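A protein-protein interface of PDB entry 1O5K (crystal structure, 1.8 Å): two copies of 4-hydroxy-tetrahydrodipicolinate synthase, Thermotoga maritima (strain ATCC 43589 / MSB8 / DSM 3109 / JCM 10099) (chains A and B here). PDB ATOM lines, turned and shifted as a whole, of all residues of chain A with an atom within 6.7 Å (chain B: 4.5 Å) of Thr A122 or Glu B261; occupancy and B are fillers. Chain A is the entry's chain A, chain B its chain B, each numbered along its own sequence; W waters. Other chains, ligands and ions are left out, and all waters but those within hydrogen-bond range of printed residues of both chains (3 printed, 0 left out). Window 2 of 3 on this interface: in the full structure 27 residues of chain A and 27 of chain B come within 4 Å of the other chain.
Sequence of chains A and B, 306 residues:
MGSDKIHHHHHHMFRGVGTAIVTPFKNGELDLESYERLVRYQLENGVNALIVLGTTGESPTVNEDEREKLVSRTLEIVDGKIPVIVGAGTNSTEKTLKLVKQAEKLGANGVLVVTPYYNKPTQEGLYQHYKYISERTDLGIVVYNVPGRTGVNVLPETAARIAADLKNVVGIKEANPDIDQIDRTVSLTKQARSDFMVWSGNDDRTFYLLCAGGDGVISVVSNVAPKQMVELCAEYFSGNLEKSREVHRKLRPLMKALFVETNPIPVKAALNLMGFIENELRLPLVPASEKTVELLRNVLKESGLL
Water W2 bridges O of Asn B263 (2.8 Å) and O of Asn A119 (2.8 Å).
Water W3 lies within hydrogen-bond range of OG1 of Thr A122 and N of Val B286.
Water W1 lies within hydrogen-bond range of O of Pro A121 (3.1 Å), OG1 of Thr B262 (3.3 Å) and O of Lys A120 (3.3 Å).
No position is printed for both chains.
Of the 6 pairs that touch across the chains among the printed residues, none has its exchanged pair printed and touching as well.
OG1 of Thr B262 sits at hydrogen-bond distance from O of Lys A120, at 2.6 Å.
The side-chain hydroxyl (OG1) of Thr A122 is in hydrogen-bond range of the backbone NH (N) of Gly A125 (3.1 Å).
OE2 of Glu B261 lies within hydrogen-bond range of N of Ser B289, at 2.9 Å.
The side-chain carboxylate (OE2) of Glu B261 is in hydrogen-bond range of the side-chain hydroxyl (OG1) of Thr B292.
Of the printed residues of chain B, Thr A122 touches Glu B261, Ile B265 and Val B286.
Glu B261 touches just one residue of chain A: Thr A122.
Of the printed residues of chain B, Asn A119 touches Thr B262 (3.3 Å).
Of the printed residues of chain B, Gly A125 touches Val B286.
Printed residues of chain B within 4 Å of Lys A120: Thr B262.
Of the printed residues of chain A, Ile B265 touches Thr A122 (3.7 Å).
Pro B266 touches none of the printed residues of chain A.
Tyr A127 touches none of the printed residues of chain B.
The nearest printed residue of chain B that does not touch Thr A122 is Thr B262 (5.0 Å).
Of the 12 printed residues of chain B, 4 touch a printed residue of chain A.
Among the printed residues, 6 pairs touch across the chains.
Among the printed residues, no Asp or Glu carboxylate lies within 4 Å of a Lys or Arg side-chain nitrogen of the other chain.
Among the printed residues, pairs that only touch across the chains: Asn A119 with Thr B262 (3.3 Å), Thr A122 with Glu B261 (3.9 Å), Thr A122 with Ile B265 (3.7 Å), Thr A122 with Val B286 (3.8 Å) and Gly A125 with Val B286 (3.96 Å).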
ATOM      1  N   ASN A 119     -17.008  20.574  -2.507  1.00  0.00           N
ATOM      2  CA  ASN A 119     -15.736  19.935  -2.870  1.00  0.00           C
ATOM      3  C   ASN A 119     -14.508  20.696  -2.391  1.00  0.00           C
ATOM      4  O   ASN A 119     -13.406  20.209  -2.621  1.00  0.00           O
ATOM      5  CB  ASN A 119     -15.674  19.598  -4.343  1.00  0.00           C
ATOM      6  CG  ASN A 119     -15.937  20.773  -5.260  1.00  0.00           C
ATOM      7  OD1 ASN A 119     -16.078  21.918  -4.835  1.00  0.00           O
ATOM      8  ND2 ASN A 119     -15.888  20.480  -6.589  1.00  0.00           N
ATOM      9  N   LYS A 120     -14.683  21.838  -1.680  1.00  0.00           N
ATOM     10  CA  LYS A 120     -13.591  22.489  -0.915  1.00  0.00           C
ATOM     11  C   LYS A 120     -12.262  22.646  -1.693  1.00  0.00           C
ATOM     12  O   LYS A 120     -11.190  22.176  -1.311  1.00  0.00           O
ATOM     13  CB  LYS A 120     -13.349  21.813   0.455  1.00  0.00           C
ATOM     14  CG  LYS A 120     -14.567  21.714   1.361  1.00  0.00           C
ATOM     15  CD  LYS A 120     -14.201  21.249   2.821  1.00  0.00           C
ATOM     16  CE  LYS A 120     -13.256  20.071   2.860  1.00  0.00           C
ATOM     17  NZ  LYS A 120     -12.876  19.627   4.267  1.00  0.00           N
ATOM     18  N   PRO A 121     -12.333  23.347  -2.799  1.00  0.00           N
ATOM     19  CA  PRO A 121     -11.124  23.570  -3.610  1.00  0.00           C
ATOM     20  C   PRO A 121     -10.056  24.351  -2.810  1.00  0.00           C
ATOM     21  O   PRO A 121     -10.368  25.133  -1.885  1.00  0.00           O
ATOM     22  CB  PRO A 121     -11.619  24.384  -4.779  1.00  0.00           C
ATOM     23  CG  PRO A 121     -12.925  24.928  -4.380  1.00  0.00           C
ATOM     24  CD  PRO A 121     -13.524  24.068  -3.304  1.00  0.00           C
ATOM     25  N   THR A 122      -8.828  24.136  -3.189  1.00  0.00           N
ATOM     26  CA  THR A 122      -7.723  24.891  -2.662  1.00  0.00           C
ATOM     27  C   THR A 122      -7.830  26.354  -3.141  1.00  0.00           C
ATOM     28  O   THR A 122      -8.593  26.663  -4.062  1.00  0.00           O
ATOM     29  CB  THR A 122      -6.433  24.280  -3.090  1.00  0.00           C
ATOM     30  OG1 THR A 122      -6.278  24.377  -4.503  1.00  0.00           O
ATOM     31  CG2 THR A 122      -6.355  22.747  -2.702  1.00  0.00           C
ATOM     32  N   GLN A 123      -7.045  27.238  -2.521  1.00  0.00           N
ATOM     33  CA  GLN A 123      -7.031  28.638  -2.922  1.00  0.00           C
ATOM     34  C   GLN A 123      -6.606  28.762  -4.400  1.00  0.00           C
ATOM     35  O   GLN A 123      -7.207  29.501  -5.168  1.00  0.00           O
ATOM     36  CB  GLN A 123      -6.126  29.475  -2.011  1.00  0.00           C
ATOM     37  CG  GLN A 123      -6.636  29.494  -0.573  1.00  0.00           C
ATOM     38  CD  GLN A 123      -7.974  30.132  -0.431  1.00  0.00           C
ATOM     39  OE1 GLN A 123      -8.117  31.306  -0.744  1.00  0.00           O
ATOM     40  NE2 GLN A 123      -8.968  29.380   0.039  1.00  0.00           N
ATOM     41  N   GLU A 124      -5.586  28.013  -4.791  1.00  0.00           N
ATOM     42  CA  GLU A 124      -5.195  27.968  -6.198  1.00  0.00           C
ATOM     43  C   GLU A 124      -6.329  27.485  -7.126  1.00  0.00           C
ATOM     44  O   GLU A 124      -6.498  28.006  -8.205  1.00  0.00           O
ATOM     45  CB  GLU A 124      -3.942  27.110  -6.373  1.00  0.00           C
ATOM     46  CG  GLU A 124      -3.415  26.988  -7.798  1.00  0.00           C
ATOM     47  CD  GLU A 124      -2.957  28.298  -8.398  1.00  0.00           C
ATOM     48  OE1 GLU A 124      -2.709  29.274  -7.651  1.00  0.00           O
ATOM     49  OE2 GLU A 124      -2.809  28.351  -9.652  1.00  0.00           O
ATOM     50  N   GLY A 125      -7.059  26.464  -6.681  1.00  0.00           N
ATOM     51  CA  GLY A 125      -8.226  25.955  -7.386  1.00  0.00           C
ATOM     52  C   GLY A 125      -9.253  27.036  -7.595  1.00  0.00           C
ATOM     53  O   GLY A 125      -9.826  27.160  -8.681  1.00  0.00           O
ATOM     54  N   LEU A 126      -9.517  27.821  -6.544  1.00  0.00           N
ATOM     55  CA  LEU A 126     -10.427  28.943  -6.695  1.00  0.00           C
ATOM     56  C   LEU A 126      -9.948  29.955  -7.728  1.00  0.00           C
ATOM     57  O   LEU A 126     -10.703  30.429  -8.547  1.00  0.00           O
ATOM     58  CB  LEU A 126     -10.619  29.659  -5.356  1.00  0.00           C
ATOM     59  CG  LEU A 126     -11.340  28.838  -4.324  1.00  0.00           C
ATOM     60  CD1 LEU A 126     -11.285  29.527  -2.949  1.00  0.00           C
ATOM     61  CD2 LEU A 126     -12.833  28.613  -4.746  1.00  0.00           C
ATOM     62  N   TYR A 127      -8.683  30.310  -7.672  1.00  0.00           N
ATOM     63  CA  TYR A 127      -8.121  31.190  -8.675  1.00  0.00           C
ATOM     64  C   TYR A 127      -8.321  30.615 -10.067  1.00  0.00           C
ATOM     65  O   TYR A 127      -8.796  31.335 -10.964  1.00  0.00           O
ATOM     66  CB  TYR A 127      -6.648  31.405  -8.390  1.00  0.00           C
ATOM     67  CG  TYR A 127      -5.961  32.265  -9.393  1.00  0.00           C
ATOM     68  CD1 TYR A 127      -6.127  33.640  -9.383  1.00  0.00           C
ATOM     69  CD2 TYR A 127      -5.134  31.717 -10.326  1.00  0.00           C
ATOM     70  CE1 TYR A 127      -5.442  34.451 -10.322  1.00  0.00           C
ATOM     71  CE2 TYR A 127      -4.462  32.506 -11.286  1.00  0.00           C
ATOM     72  CZ  TYR A 127      -4.631  33.880 -11.272  1.00  0.00           C
ATOM     73  OH  TYR A 127      -3.920  34.663 -12.198  1.00  0.00           O
ATOM     74  N   VAL A 152     -15.732  26.524   2.187  1.00  0.00           N
ATOM     75  CA  VAL A 152     -14.447  27.086   1.759  1.00  0.00           C
ATOM     76  C   VAL A 152     -14.542  28.590   1.901  1.00  0.00           C
ATOM     77  O   VAL A 152     -15.614  29.183   1.636  1.00  0.00           O
ATOM     78  CB  VAL A 152     -14.107  26.702   0.302  1.00  0.00           C
ATOM     79  CG1 VAL A 152     -15.034  27.408  -0.702  1.00  0.00           C
ATOM     80  CG2 VAL A 152     -12.657  27.057   0.037  1.00  0.00           C
ATOM     81  N   THR A 158      -6.279  35.947  -1.818  1.00  0.00           N
ATOM     82  CA  THR A 158      -6.740  35.225  -3.015  1.00  0.00           C
ATOM     83  C   THR A 158      -7.704  36.124  -3.754  1.00  0.00           C
ATOM     84  O   THR A 158      -7.581  36.282  -4.953  1.00  0.00           O
ATOM     85  CB  THR A 158      -7.400  33.908  -2.665  1.00  0.00           C
ATOM     86  OG1 THR A 158      -6.497  33.077  -1.963  1.00  0.00           O
ATOM     87  CG2 THR A 158      -7.773  33.124  -3.892  1.00  0.00           C
ATOM     88  N   LEU B 258      -3.422  11.984   3.942  1.00  0.00           N
ATOM     89  CA  LEU B 258      -4.404  11.991   2.875  1.00  0.00           C
ATOM     90  C   LEU B 258      -5.411  13.141   2.965  1.00  0.00           C
ATOM     91  O   LEU B 258      -6.229  13.330   2.077  1.00  0.00           O
ATOM     92  CB  LEU B 258      -5.097  10.612   2.773  1.00  0.00           C
ATOM     93  CG  LEU B 258      -4.195   9.503   2.254  1.00  0.00           C
ATOM     94  CD1 LEU B 258      -4.962   8.211   2.220  1.00  0.00           C
ATOM     95  CD2 LEU B 258      -3.666   9.780   0.861  1.00  0.00           C
ATOM     96  N   PHE B 259      -5.320  13.950   4.022  1.00  0.00           N
ATOM     97  CA  PHE B 259      -6.155  15.120   4.159  1.00  0.00           C
ATOM     98  C   PHE B 259      -5.388  16.414   4.370  1.00  0.00           C
ATOM     99  O   PHE B 259      -5.983  17.410   4.725  1.00  0.00           O
ATOM    100  CB  PHE B 259      -7.196  14.870   5.244  1.00  0.00           C
ATOM    101  CG  PHE B 259      -8.069  13.749   4.901  1.00  0.00           C
ATOM    102  CD1 PHE B 259      -9.203  13.953   4.136  1.00  0.00           C
ATOM    103  CD2 PHE B 259      -7.702  12.453   5.236  1.00  0.00           C
ATOM    104  CE1 PHE B 259      -9.989  12.878   3.779  1.00  0.00           C
ATOM    105  CE2 PHE B 259      -8.463  11.383   4.861  1.00  0.00           C
ATOM    106  CZ  PHE B 259      -9.599  11.591   4.124  1.00  0.00           C
ATOM    107  N   VAL B 260      -4.080  16.449   4.092  1.00  0.00           N
ATOM    108  CA  VAL B 260      -3.386  17.720   4.203  1.00  0.00           C
ATOM    109  C   VAL B 260      -3.854  18.759   3.172  1.00  0.00           C
ATOM    110  O   VAL B 260      -3.682  19.967   3.392  1.00  0.00           O
ATOM    111  CB  VAL B 260      -1.881  17.602   4.124  1.00  0.00           C
ATOM    112  CG1 VAL B 260      -1.395  16.863   5.361  1.00  0.00           C
ATOM    113  CG2 VAL B 260      -1.412  16.932   2.837  1.00  0.00           C
ATOM    114  N   GLU B 261      -4.380  18.282   2.050  1.00  0.00           N
ATOM    115  CA  GLU B 261      -5.139  19.114   1.117  1.00  0.00           C
ATOM    116  C   GLU B 261      -6.445  18.374   0.930  1.00  0.00           C
ATOM    117  O   GLU B 261      -6.581  17.226   1.315  1.00  0.00           O
ATOM    118  CB  GLU B 261      -4.431  19.305  -0.230  1.00  0.00           C
ATOM    119  CG  GLU B 261      -3.112  20.042  -0.154  1.00  0.00           C
ATOM    120  CD  GLU B 261      -2.422  20.194  -1.514  1.00  0.00           C
ATOM    121  OE1 GLU B 261      -2.885  20.961  -2.343  1.00  0.00           O
ATOM    122  OE2 GLU B 261      -1.399  19.534  -1.773  1.00  0.00           O
ATOM    123  N   THR B 262      -7.445  19.075   0.435  1.00  0.00           N
ATOM    124  CA  THR B 262      -8.771  18.546   0.332  1.00  0.00           C
ATOM    125  C   THR B 262      -8.790  17.229  -0.406  1.00  0.00           C
ATOM    126  O   THR B 262      -8.229  17.133  -1.516  1.00  0.00           O
ATOM    127  CB  THR B 262      -9.650  19.552  -0.450  1.00  0.00           C
ATOM    128  OG1 THR B 262      -9.815  20.749   0.325  1.00  0.00           O
ATOM    129  CG2 THR B 262     -11.034  18.991  -0.677  1.00  0.00           C
ATOM    130  N   ASN B 263      -9.410  16.209   0.193  1.00  0.00           N
ATOM    131  CA  ASN B 263      -9.623  14.918  -0.491  1.00  0.00           C
ATOM    132  C   ASN B 263     -10.475  15.110  -1.727  1.00  0.00           C
ATOM    133  O   ASN B 263     -11.433  15.849  -1.651  1.00  0.00           O
ATOM    134  CB  ASN B 263     -10.286  13.967   0.522  1.00  0.00           C
ATOM    135  CG  ASN B 263     -10.725  12.691  -0.060  1.00  0.00           C
ATOM    136  OD1 ASN B 263     -11.924  12.355  -0.010  1.00  0.00           O
ATOM    137  ND2 ASN B 263      -9.803  11.948  -0.588  1.00  0.00           N
ATOM    138  N   ILE B 265      -7.366  15.227  -3.522  1.00  0.00           N
ATOM    139  CA  ILE B 265      -6.106  15.697  -4.084  1.00  0.00           C
ATOM    140  C   ILE B 265      -4.927  14.831  -3.612  1.00  0.00           C
ATOM    141  O   ILE B 265      -4.159  14.301  -4.451  1.00  0.00           O
ATOM    142  CB  ILE B 265      -5.909  17.218  -3.819  1.00  0.00           C
ATOM    143  CG1 ILE B 265      -6.929  18.019  -4.646  1.00  0.00           C
ATOM    144  CG2 ILE B 265      -4.502  17.703  -4.165  1.00  0.00           C
ATOM    145  CD1 ILE B 265      -7.034  19.482  -4.213  1.00  0.00           C
ATOM    146  N   PRO B 266      -4.769  14.619  -2.298  1.00  0.00           N
ATOM    147  CA  PRO B 266      -3.649  13.762  -1.847  1.00  0.00           C
ATOM    148  C   PRO B 266      -3.771  12.294  -2.286  1.00  0.00           C
ATOM    149  O   PRO B 266      -2.795  11.664  -2.712  1.00  0.00           O
ATOM    150  CB  PRO B 266      -3.737  13.885  -0.319  1.00  0.00           C
ATOM    151  CG  PRO B 266      -4.400  15.203  -0.066  1.00  0.00           C
ATOM    152  CD  PRO B 266      -5.467  15.226  -1.142  1.00  0.00           C
ATOM    153  N   VAL B 286      -7.170  20.665  -8.218  1.00  0.00           N
ATOM    154  CA  VAL B 286      -5.872  20.758  -8.929  1.00  0.00           C
ATOM    155  C   VAL B 286      -4.942  19.773  -8.227  1.00  0.00           C
ATOM    156  O   VAL B 286      -5.224  19.379  -7.080  1.00  0.00           O
ATOM    157  CB  VAL B 286      -5.251  22.186  -8.889  1.00  0.00           C
ATOM    158  CG1 VAL B 286      -6.216  23.219  -9.427  1.00  0.00           C
ATOM    159  CG2 VAL B 286      -4.875  22.579  -7.493  1.00  0.00           C
ATOM    160  N   ALA B 288      -1.911  17.897  -6.164  1.00  0.00           N
ATOM    161  CA  ALA B 288      -1.222  18.144  -4.899  1.00  0.00           C
ATOM    162  C   ALA B 288       0.049  18.982  -5.039  1.00  0.00           C
ATOM    163  O   ALA B 288       0.773  18.858  -6.031  1.00  0.00           O
ATOM    164  CB  ALA B 288      -0.866  16.799  -4.267  1.00  0.00           C
ATOM    165  N   SER B 289       0.347  19.784  -4.016  1.00  0.00           N
ATOM    166  CA  SER B 289       1.589  20.586  -3.978  1.00  0.00           C
ATOM    167  C   SER B 289       2.803  19.648  -3.889  1.00  0.00           C
ATOM    168  O   SER B 289       2.634  18.472  -3.510  1.00  0.00           O
ATOM    169  CB  SER B 289       1.531  21.488  -2.730  1.00  0.00           C
ATOM    170  OG  SER B 289       1.702  20.696  -1.563  1.00  0.00           O
ATOM    171  N   THR B 292       3.051  18.283  -0.456  1.00  0.00           N
ATOM    172  CA  THR B 292       2.140  17.162  -0.227  1.00  0.00           C
ATOM    173  C   THR B 292       2.706  15.876  -0.792  1.00  0.00           C
ATOM    174  O   THR B 292       2.637  14.831  -0.161  1.00  0.00           O
ATOM    175  CB  THR B 292       0.781  17.482  -0.811  1.00  0.00           C
ATOM    176  OG1 THR B 292       0.158  18.479   0.022  1.00  0.00           O
ATOM    177  CG2 THR B 292      -0.162  16.262  -0.735  1.00  0.00           C
HETATM  178  O   HOH W   1      -9.319  23.964   0.753  1.00  0.00           O
HETATM  179  O   HOH W   2     -13.395  17.425  -2.787  1.00  0.00           O
HETATM  180  O   HOH W   3      -8.319  22.745  -5.691  1.00  0.00           O
